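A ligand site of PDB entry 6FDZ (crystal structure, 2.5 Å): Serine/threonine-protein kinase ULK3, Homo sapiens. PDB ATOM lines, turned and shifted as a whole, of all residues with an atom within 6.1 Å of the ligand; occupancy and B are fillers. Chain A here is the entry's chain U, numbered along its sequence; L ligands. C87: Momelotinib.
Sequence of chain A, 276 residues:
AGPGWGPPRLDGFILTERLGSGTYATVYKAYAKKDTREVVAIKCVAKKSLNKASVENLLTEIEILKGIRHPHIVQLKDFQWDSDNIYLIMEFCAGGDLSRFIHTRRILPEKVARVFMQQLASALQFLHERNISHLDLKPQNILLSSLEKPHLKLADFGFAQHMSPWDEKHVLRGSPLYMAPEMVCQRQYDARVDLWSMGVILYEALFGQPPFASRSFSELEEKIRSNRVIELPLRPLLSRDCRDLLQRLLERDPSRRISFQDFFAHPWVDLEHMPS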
ATOM      1  N   ARG A  18     -11.331  16.298  19.959  1.00  0.00           N
ATOM      2  CA  ARG A  18      -9.959  16.667  19.746  1.00  0.00           C
ATOM      3  C   ARG A  18      -9.130  15.800  20.727  1.00  0.00           C
ATOM      4  O   ARG A  18      -9.474  15.671  21.910  1.00  0.00           O
ATOM      5  CB  ARG A  18      -9.835  18.174  20.013  1.00  0.00           C
ATOM      6  CG  ARG A  18      -8.529  18.854  19.621  1.00  0.00           C
ATOM      7  CD  ARG A  18      -8.579  20.314  20.080  1.00  0.00           C
ATOM      8  NE  ARG A  18      -9.507  21.089  19.240  1.00  0.00           N
ATOM      9  CZ  ARG A  18     -10.570  21.793  19.643  1.00  0.00           C
ATOM     10  NH1 ARG A  18     -10.921  21.896  20.929  1.00  0.00           N
ATOM     11  NH2 ARG A  18     -11.305  22.438  18.740  1.00  0.00           N
ATOM     12  N   LEU A  19      -8.094  15.155  20.212  1.00  0.00           N
ATOM     13  CA  LEU A  19      -7.191  14.322  20.982  1.00  0.00           C
ATOM     14  C   LEU A  19      -5.810  14.952  21.157  1.00  0.00           C
ATOM     15  O   LEU A  19      -5.044  14.599  22.088  1.00  0.00           O
ATOM     16  CB  LEU A  19      -7.023  12.975  20.231  1.00  0.00           C
ATOM     17  CG  LEU A  19      -8.283  12.119  19.959  1.00  0.00           C
ATOM     18  CD1 LEU A  19      -7.977  10.990  18.984  1.00  0.00           C
ATOM     19  CD2 LEU A  19      -8.865  11.563  21.247  1.00  0.00           C
ATOM     20  N   GLY A  20      -5.453  15.834  20.237  1.00  0.00           N
ATOM     21  CA  GLY A  20      -4.101  16.393  20.173  1.00  0.00           C
ATOM     22  C   GLY A  20      -4.071  17.631  19.304  1.00  0.00           C
ATOM     23  O   GLY A  20      -4.919  17.827  18.446  1.00  0.00           O
ATOM     24  N   SER A  21      -3.087  18.478  19.575  1.00  0.00           N
ATOM     25  CA  SER A  21      -2.930  19.794  18.951  1.00  0.00           C
ATOM     26  C   SER A  21      -1.446  20.046  18.866  1.00  0.00           C
ATOM     27  O   SER A  21      -0.682  19.678  19.774  1.00  0.00           O
ATOM     28  CB  SER A  21      -3.622  20.898  19.738  1.00  0.00           C
ATOM     29  N   GLY A  22      -1.019  20.577  17.731  1.00  0.00           N
ATOM     30  CA  GLY A  22       0.326  21.068  17.543  1.00  0.00           C
ATOM     31  C   GLY A  22       0.215  22.500  17.038  1.00  0.00           C
ATOM     32  O   GLY A  22      -0.887  22.971  16.675  1.00  0.00           O
ATOM     33  N   TYR A  24       0.891  23.427  14.250  1.00  0.00           N
ATOM     34  CA  TYR A  24       0.338  23.264  12.896  1.00  0.00           C
ATOM     35  C   TYR A  24      -0.737  22.176  12.679  1.00  0.00           C
ATOM     36  O   TYR A  24      -1.472  22.241  11.687  1.00  0.00           O
ATOM     37  CB  TYR A  24       1.499  23.026  11.917  1.00  0.00           C
ATOM     38  CG  TYR A  24       2.415  24.244  11.825  1.00  0.00           C
ATOM     39  CD1 TYR A  24       1.958  25.462  11.244  1.00  0.00           C
ATOM     40  CD2 TYR A  24       3.726  24.207  12.334  1.00  0.00           C
ATOM     41  CE1 TYR A  24       2.782  26.578  11.164  1.00  0.00           C
ATOM     42  CE2 TYR A  24       4.550  25.339  12.261  1.00  0.00           C
ATOM     43  CZ  TYR A  24       4.071  26.520  11.679  1.00  0.00           C
ATOM     44  OH  TYR A  24       4.881  27.636  11.601  1.00  0.00           O
ATOM     45  N   ALA A  25      -0.827  21.186  13.567  1.00  0.00           N
ATOM     46  CA  ALA A  25      -1.683  19.994  13.344  1.00  0.00           C
ATOM     47  C   ALA A  25      -2.707  19.773  14.417  1.00  0.00           C
ATOM     48  O   ALA A  25      -2.584  20.248  15.519  1.00  0.00           O
ATOM     49  CB  ALA A  25      -0.813  18.745  13.212  1.00  0.00           C
ATOM     50  N   THR A  26      -3.707  19.003  14.099  1.00  0.00           N
ATOM     51  CA  THR A  26      -4.723  18.680  15.069  1.00  0.00           C
ATOM     52  C   THR A  26      -5.166  17.261  14.789  1.00  0.00           C
ATOM     53  O   THR A  26      -5.425  16.908  13.643  1.00  0.00           O
ATOM     54  CB  THR A  26      -5.938  19.592  14.916  1.00  0.00           C
ATOM     55  OG1 THR A  26      -5.494  20.948  14.840  1.00  0.00           O
ATOM     56  CG2 THR A  26      -6.921  19.396  16.080  1.00  0.00           C
ATOM     57  N   VAL A  27      -5.301  16.485  15.863  1.00  0.00           N
ATOM     58  CA  VAL A  27      -5.692  15.100  15.744  1.00  0.00           C
ATOM     59  C   VAL A  27      -7.061  14.923  16.347  1.00  0.00           C
ATOM     60  O   VAL A  27      -7.234  15.152  17.524  1.00  0.00           O
ATOM     61  CB  VAL A  27      -4.687  14.207  16.454  1.00  0.00           C
ATOM     62  CG1 VAL A  27      -5.106  12.748  16.351  1.00  0.00           C
ATOM     63  CG2 VAL A  27      -3.295  14.453  15.865  1.00  0.00           C
ATOM     64  N   ALA A  41      -8.168   7.521  14.510  1.00  0.00           N
ATOM     65  CA  ALA A  41      -7.631   8.850  14.849  1.00  0.00           C
ATOM     66  C   ALA A  41      -7.157   9.487  13.525  1.00  0.00           C
ATOM     67  O   ALA A  41      -6.464   8.834  12.699  1.00  0.00           O
ATOM     68  CB  ALA A  41      -6.471   8.717  15.826  1.00  0.00           C
ATOM     69  N   LYS A  43      -5.022  12.660  11.978  1.00  0.00           N
ATOM     70  CA  LYS A  43      -4.182  13.864  12.052  1.00  0.00           C
ATOM     71  C   LYS A  43      -4.386  14.791  10.842  1.00  0.00           C
ATOM     72  O   LYS A  43      -4.144  14.390   9.670  1.00  0.00           O
ATOM     73  CB  LYS A  43      -2.705  13.511  12.156  1.00  0.00           C
ATOM     74  CG  LYS A  43      -1.842  14.715  12.506  1.00  0.00           C
ATOM     75  CD  LYS A  43      -0.449  14.343  12.990  1.00  0.00           C
ATOM     76  CE  LYS A  43       0.305  15.542  13.543  1.00  0.00           C
ATOM     77  NZ  LYS A  43       1.462  15.117  14.379  1.00  0.00           N
ATOM     78  N   CYS A  44      -4.780  16.037  11.132  1.00  0.00           N
ATOM     79  CA  CYS A  44      -5.008  17.067  10.118  1.00  0.00           C
ATOM     80  C   CYS A  44      -3.940  18.162  10.105  1.00  0.00           C
ATOM     81  O   CYS A  44      -3.701  18.807  11.115  1.00  0.00           O
ATOM     82  CB  CYS A  44      -6.359  17.711  10.333  1.00  0.00           C
ATOM     83  SG  CYS A  44      -7.631  16.471  10.646  1.00  0.00           S
ATOM     84  N   VAL A  74       1.409   1.902  15.902  1.00  0.00           N
ATOM     85  CA  VAL A  74       0.148   2.459  15.476  1.00  0.00           C
ATOM     86  C   VAL A  74       0.204   2.399  13.977  1.00  0.00           C
ATOM     87  O   VAL A  74       1.226   2.757  13.339  1.00  0.00           O
ATOM     88  CB  VAL A  74      -0.050   3.924  15.933  1.00  0.00           C
ATOM     89  CG1 VAL A  74      -1.364   4.480  15.435  1.00  0.00           C
ATOM     90  CG2 VAL A  74       0.009   4.014  17.455  1.00  0.00           C
ATOM     91  N   MET A  90      -5.261   7.034  11.141  1.00  0.00           N
ATOM     92  CA  MET A  90      -4.518   6.081  11.972  1.00  0.00           C
ATOM     93  C   MET A  90      -5.441   5.172  12.784  1.00  0.00           C
ATOM     94  O   MET A  90      -6.570   5.537  13.072  1.00  0.00           O
ATOM     95  CB  MET A  90      -3.637   6.866  12.946  1.00  0.00           C
ATOM     96  CG  MET A  90      -2.532   7.698  12.358  1.00  0.00           C
ATOM     97  SD  MET A  90      -1.865   8.812  13.613  1.00  0.00           S
ATOM     98  CE  MET A  90      -3.243   9.923  13.797  1.00  0.00           C
ATOM     99  N   GLU A  91      -4.923   4.011  13.173  1.00  0.00           N
ATOM    100  CA  GLU A  91      -5.509   3.140  14.176  1.00  0.00           C
ATOM    101  C   GLU A  91      -5.765   3.934  15.440  1.00  0.00           C
ATOM    102  O   GLU A  91      -4.853   4.549  15.965  1.00  0.00           O
ATOM    103  CB  GLU A  91      -4.500   2.010  14.481  1.00  0.00           C
ATOM    104  CG  GLU A  91      -4.891   1.032  15.567  1.00  0.00           C
ATOM    105  CD  GLU A  91      -3.749   0.078  15.953  1.00  0.00           C
ATOM    106  OE1 GLU A  91      -2.640  -0.018  15.290  1.00  0.00           O
ATOM    107  OE2 GLU A  91      -4.001  -0.613  16.962  1.00  0.00           O
ATOM    108  N   PHE A  92      -6.984   3.956  15.921  1.00  0.00           N
ATOM    109  CA  PHE A  92      -7.312   4.629  17.184  1.00  0.00           C
ATOM    110  C   PHE A  92      -6.902   3.761  18.385  1.00  0.00           C
ATOM    111  O   PHE A  92      -7.274   2.609  18.444  1.00  0.00           O
ATOM    112  CB  PHE A  92      -8.794   4.942  17.241  1.00  0.00           C
ATOM    113  CG  PHE A  92      -9.256   5.504  18.524  1.00  0.00           C
ATOM    114  CD1 PHE A  92      -8.800   6.749  18.940  1.00  0.00           C
ATOM    115  CD2 PHE A  92     -10.150   4.815  19.327  1.00  0.00           C
ATOM    116  CE1 PHE A  92      -9.237   7.297  20.164  1.00  0.00           C
ATOM    117  CE2 PHE A  92     -10.602   5.364  20.534  1.00  0.00           C
ATOM    118  CZ  PHE A  92     -10.145   6.610  20.949  1.00  0.00           C
ATOM    119  N   CYS A  93      -6.152   4.336  19.317  1.00  0.00           N
ATOM    120  CA  CYS A  93      -5.807   3.759  20.587  1.00  0.00           C
ATOM    121  C   CYS A  93      -6.623   4.425  21.732  1.00  0.00           C
ATOM    122  O   CYS A  93      -6.390   5.580  22.093  1.00  0.00           O
ATOM    123  CB  CYS A  93      -4.321   3.901  20.792  1.00  0.00           C
ATOM    124  SG  CYS A  93      -3.361   3.211  19.435  1.00  0.00           S
ATOM    125  N   ALA A  94      -7.544   3.673  22.308  1.00  0.00           N
ATOM    126  CA  ALA A  94      -8.537   4.182  23.219  1.00  0.00           C
ATOM    127  C   ALA A  94      -8.037   4.317  24.644  1.00  0.00           C
ATOM    128  O   ALA A  94      -8.753   4.878  25.438  1.00  0.00           O
ATOM    129  CB  ALA A  94      -9.761   3.285  23.215  1.00  0.00           C
ATOM    130  N   GLY A  95      -6.854   3.774  24.964  1.00  0.00           N
ATOM    131  CA  GLY A  95      -6.247   3.937  26.280  1.00  0.00           C
ATOM    132  C   GLY A  95      -5.424   5.198  26.537  1.00  0.00           C
ATOM    133  O   GLY A  95      -4.947   5.432  27.672  1.00  0.00           O
ATOM    134  N   GLY A  96      -5.236   6.024  25.520  1.00  0.00           N
ATOM    135  CA  GLY A  96      -4.447   7.224  25.683  1.00  0.00           C
ATOM    136  C   GLY A  96      -2.986   6.882  25.748  1.00  0.00           C
ATOM    137  O   GLY A  96      -2.583   5.779  25.365  1.00  0.00           O
ATOM    138  N   ASP A  97      -2.186   7.809  26.264  1.00  0.00           N
ATOM    139  CA  ASP A  97      -0.748   7.687  26.154  1.00  0.00           C
ATOM    140  C   ASP A  97      -0.174   6.985  27.364  1.00  0.00           C
ATOM    141  O   ASP A  97      -0.823   6.986  28.414  1.00  0.00           O
ATOM    142  CB  ASP A  97      -0.079   9.043  25.827  1.00  0.00           C
ATOM    143  CG  ASP A  97      -0.078  10.008  26.974  1.00  0.00           C
ATOM    144  OD1 ASP A  97       0.709   9.807  27.882  1.00  0.00           O
ATOM    145  OD2 ASP A  97      -0.802  11.000  26.960  1.00  0.00           O
ATOM    146  N   ARG A 100       0.418   9.392  30.780  1.00  0.00           N
ATOM    147  CA  ARG A 100      -0.711   9.488  31.722  1.00  0.00           C
ATOM    148  C   ARG A 100      -0.803   8.148  32.492  1.00  0.00           C
ATOM    149  O   ARG A 100      -0.930   8.129  33.742  1.00  0.00           O
ATOM    150  CB  ARG A 100      -2.067   9.792  31.002  1.00  0.00           C
ATOM    151  CG  ARG A 100      -2.438  11.277  30.664  1.00  0.00           C
ATOM    152  CD  ARG A 100      -3.987  11.506  30.687  1.00  0.00           C
ATOM    153  NE  ARG A 100      -4.471  12.884  30.484  1.00  0.00           N
ATOM    154  N   LEU A 143       1.222   4.740  22.888  1.00  0.00           N
ATOM    155  CA  LEU A 143      -0.220   4.682  23.199  1.00  0.00           C
ATOM    156  C   LEU A 143      -0.702   3.280  23.594  1.00  0.00           C
ATOM    157  O   LEU A 143       0.011   2.281  23.412  1.00  0.00           O
ATOM    158  CB  LEU A 143      -1.056   5.185  22.023  1.00  0.00           C
ATOM    159  CG  LEU A 143      -0.718   6.583  21.462  1.00  0.00           C
ATOM    160  CD1 LEU A 143      -1.503   6.885  20.194  1.00  0.00           C
ATOM    161  CD2 LEU A 143      -0.984   7.665  22.508  1.00  0.00           C
ATOM    162  N   ALA A 155       3.921   5.355  18.467  1.00  0.00           N
ATOM    163  CA  ALA A 155       3.347   6.422  17.602  1.00  0.00           C
ATOM    164  C   ALA A 155       4.423   7.402  17.115  1.00  0.00           C
ATOM    165  O   ALA A 155       5.499   7.510  17.712  1.00  0.00           O
ATOM    166  CB  ALA A 155       2.239   7.173  18.340  1.00  0.00           C
ATOM    167  N   ASP A 156       4.132   8.093  16.021  1.00  0.00           N
ATOM    168  CA  ASP A 156       5.021   9.126  15.477  1.00  0.00           C
ATOM    169  C   ASP A 156       4.277  10.440  15.575  1.00  0.00           C
ATOM    170  O   ASP A 156       3.424  10.744  14.740  1.00  0.00           O
ATOM    171  CB  ASP A 156       5.404   8.792  14.034  1.00  0.00           C
ATOM    172  CG  ASP A 156       6.644   9.536  13.579  1.00  0.00           C
ATOM    173  OD1 ASP A 156       6.855  10.679  14.051  1.00  0.00           O
ATOM    174  OD2 ASP A 156       7.415   8.959  12.758  1.00  0.00           O
ATOM    175  N   PHE A 157       4.583  11.201  16.633  1.00  0.00           N
ATOM    176  CA  PHE A 157       3.908  12.472  16.957  1.00  0.00           C
ATOM    177  C   PHE A 157       4.470  13.626  16.136  1.00  0.00           C
ATOM    178  O   PHE A 157       3.967  14.725  16.258  1.00  0.00           O
ATOM    179  CB  PHE A 157       4.024  12.816  18.465  1.00  0.00           C
ATOM    180  CG  PHE A 157       2.887  12.278  19.328  1.00  0.00           C
ATOM    181  CD1 PHE A 157       2.284  11.035  19.071  1.00  0.00           C
ATOM    182  CD2 PHE A 157       2.437  13.007  20.427  1.00  0.00           C
ATOM    183  CE1 PHE A 157       1.249  10.553  19.867  1.00  0.00           C
ATOM    184  CE2 PHE A 157       1.396  12.537  21.223  1.00  0.00           C
ATOM    185  CZ  PHE A 157       0.806  11.295  20.949  1.00  0.00           C
ATOM    186  N   GLY A 158       5.515  13.381  15.354  1.00  0.00           N
ATOM    187  CA  GLY A 158       6.179  14.409  14.591  1.00  0.00           C
ATOM    188  C   GLY A 158       6.371  13.957  13.160  1.00  0.00           C
ATOM    189  O   GLY A 158       7.480  13.596  12.769  1.00  0.00           O
HETATM  190  O23 C87 L   1       0.741  13.869  16.670  1.00  0.00           O
HETATM  191  C22 C87 L   1      -0.026  13.843  17.627  1.00  0.00           C
HETATM  192  N24 C87 L   1      -0.178  14.892  18.451  1.00  0.00           N
HETATM  193  C25 C87 L   1       0.451  16.174  18.158  1.00  0.00           C
HETATM  194  C26 C87 L   1      -0.324  16.902  17.145  1.00  0.00           C
HETATM  195  N27 C87 L   1      -0.947  17.432  16.352  1.00  0.00           N
HETATM  196  C19 C87 L   1      -0.861  12.625  17.899  1.00  0.00           C
HETATM  197  C18 C87 L   1      -0.679  11.492  17.111  1.00  0.00           C
HETATM  198  C17 C87 L   1      -1.523  10.404  17.216  1.00  0.00           C
HETATM  199  C16 C87 L   1      -2.560  10.381  18.153  1.00  0.00           C
HETATM  200  C21 C87 L   1      -2.735  11.518  18.947  1.00  0.00           C
HETATM  201  C20 C87 L   1      -1.906  12.615  18.821  1.00  0.00           C
HETATM  202  C12 C87 L   1      -3.384   9.165  18.373  1.00  0.00           C
HETATM  203  C11 C87 L   1      -3.348   8.070  17.519  1.00  0.00           C
HETATM  204  C10 C87 L   1      -4.158   7.001  17.837  1.00  0.00           C
HETATM  205  N15 C87 L   1      -4.962   6.971  18.900  1.00  0.00           N
HETATM  206  C14 C87 L   1      -4.896   8.048  19.684  1.00  0.00           C
HETATM  207  N13 C87 L   1      -4.165   9.154  19.465  1.00  0.00           N
HETATM  208  N7  C87 L   1      -5.538   7.872  20.865  1.00  0.00           N
HETATM  209  C1  C87 L   1      -5.641   8.742  21.961  1.00  0.00           C
HETATM  210  C2  C87 L   1      -6.734   8.630  22.800  1.00  0.00           C
HETATM  211  C3  C87 L   1      -6.872   9.488  23.881  1.00  0.00           C
HETATM  212  C4  C87 L   1      -5.917  10.483  24.124  1.00  0.00           C
HETATM  213  C5  C87 L   1      -4.810  10.570  23.284  1.00  0.00           C
HETATM  214  C6  C87 L   1      -4.664   9.699  22.219  1.00  0.00           C
HETATM  215  N8  C87 L   1      -6.078  11.395  25.180  1.00  0.00           N
HETATM  216  C28 C87 L   1      -7.083  11.131  26.221  1.00  0.00           C
HETATM  217  C29 C87 L   1      -6.725  11.900  27.455  1.00  0.00           C
HETATM  218  O30 C87 L   1      -6.626  13.281  27.173  1.00  0.00           O
HETATM  219  C31 C87 L   1      -5.572  13.491  26.249  1.00  0.00           C
HETATM  220  C9  C87 L   1      -5.863  12.821  24.946  1.00  0.00           C
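O of Ala 25 sits close to N27 of the ligand. The backbone carbonyl oxygen (O) of Phe 157 lies close to an oxygen (O23) of the ligand (3.4 Å). Residues that only touch the ligand: Leu 19, Ser 21, Thr 26, Val 27, Ala 41, Met 90, Glu 91, Phe 92, Gly 96, Arg 100 and Leu 143. Hydrophobic or aromatic side chains that line the ligand: Leu 19, Ala 25, Val 27, Ala 41, Met 90, Phe 92, Leu 143 and Phe 157. Within 4 Å of the ligand: Leu 19, Ser 21, Gly 22, Ala 25, Thr 26, Val 27, Ala 41, Lys 43, Met 90, Glu 91, Phe 92, Cys 93, Gly 96, Arg 100, Leu 143 and Phe 157.
The side-chain amino group (NZ) of Lys 43 lies within hydrogen-bond range of the backbone carbonyl oxygen (O) of Phe 157 (3.2 Å). The side-chain carboxylate of Asp 97 sits at hydrogen-bond distance from the backbone NH of Arg 100. N of Leu 19 is in hydrogen-bond range of O of Val 27, 2.8 Å away. N of Val 27 lies within hydrogen-bond range of O of Gly 20 (2.9 Å). O of Ala 41 lies within hydrogen-bond range of N of Met 90, 2.7 Å away. O of Thr 26 sits at hydrogen-bond distance from N of Cys 44 (2.7 Å).
The backbone NH of Cys 93 lies within hydrogen-bond range of a nitrogen (N15) of the ligand (2.9 Å). The backbone NH (N) of Gly 22 is in hydrogen-bond range of a nitrogen (N27) of the ligand. O23 of the ligand is in hydrogen-bond range of NZ of Lys 43 (2.7 Å). The backbone carbonyl oxygen of Cys 93 sits at hydrogen-bond distance from a nitrogen (N7) of the ligand, 2.7 Å away.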
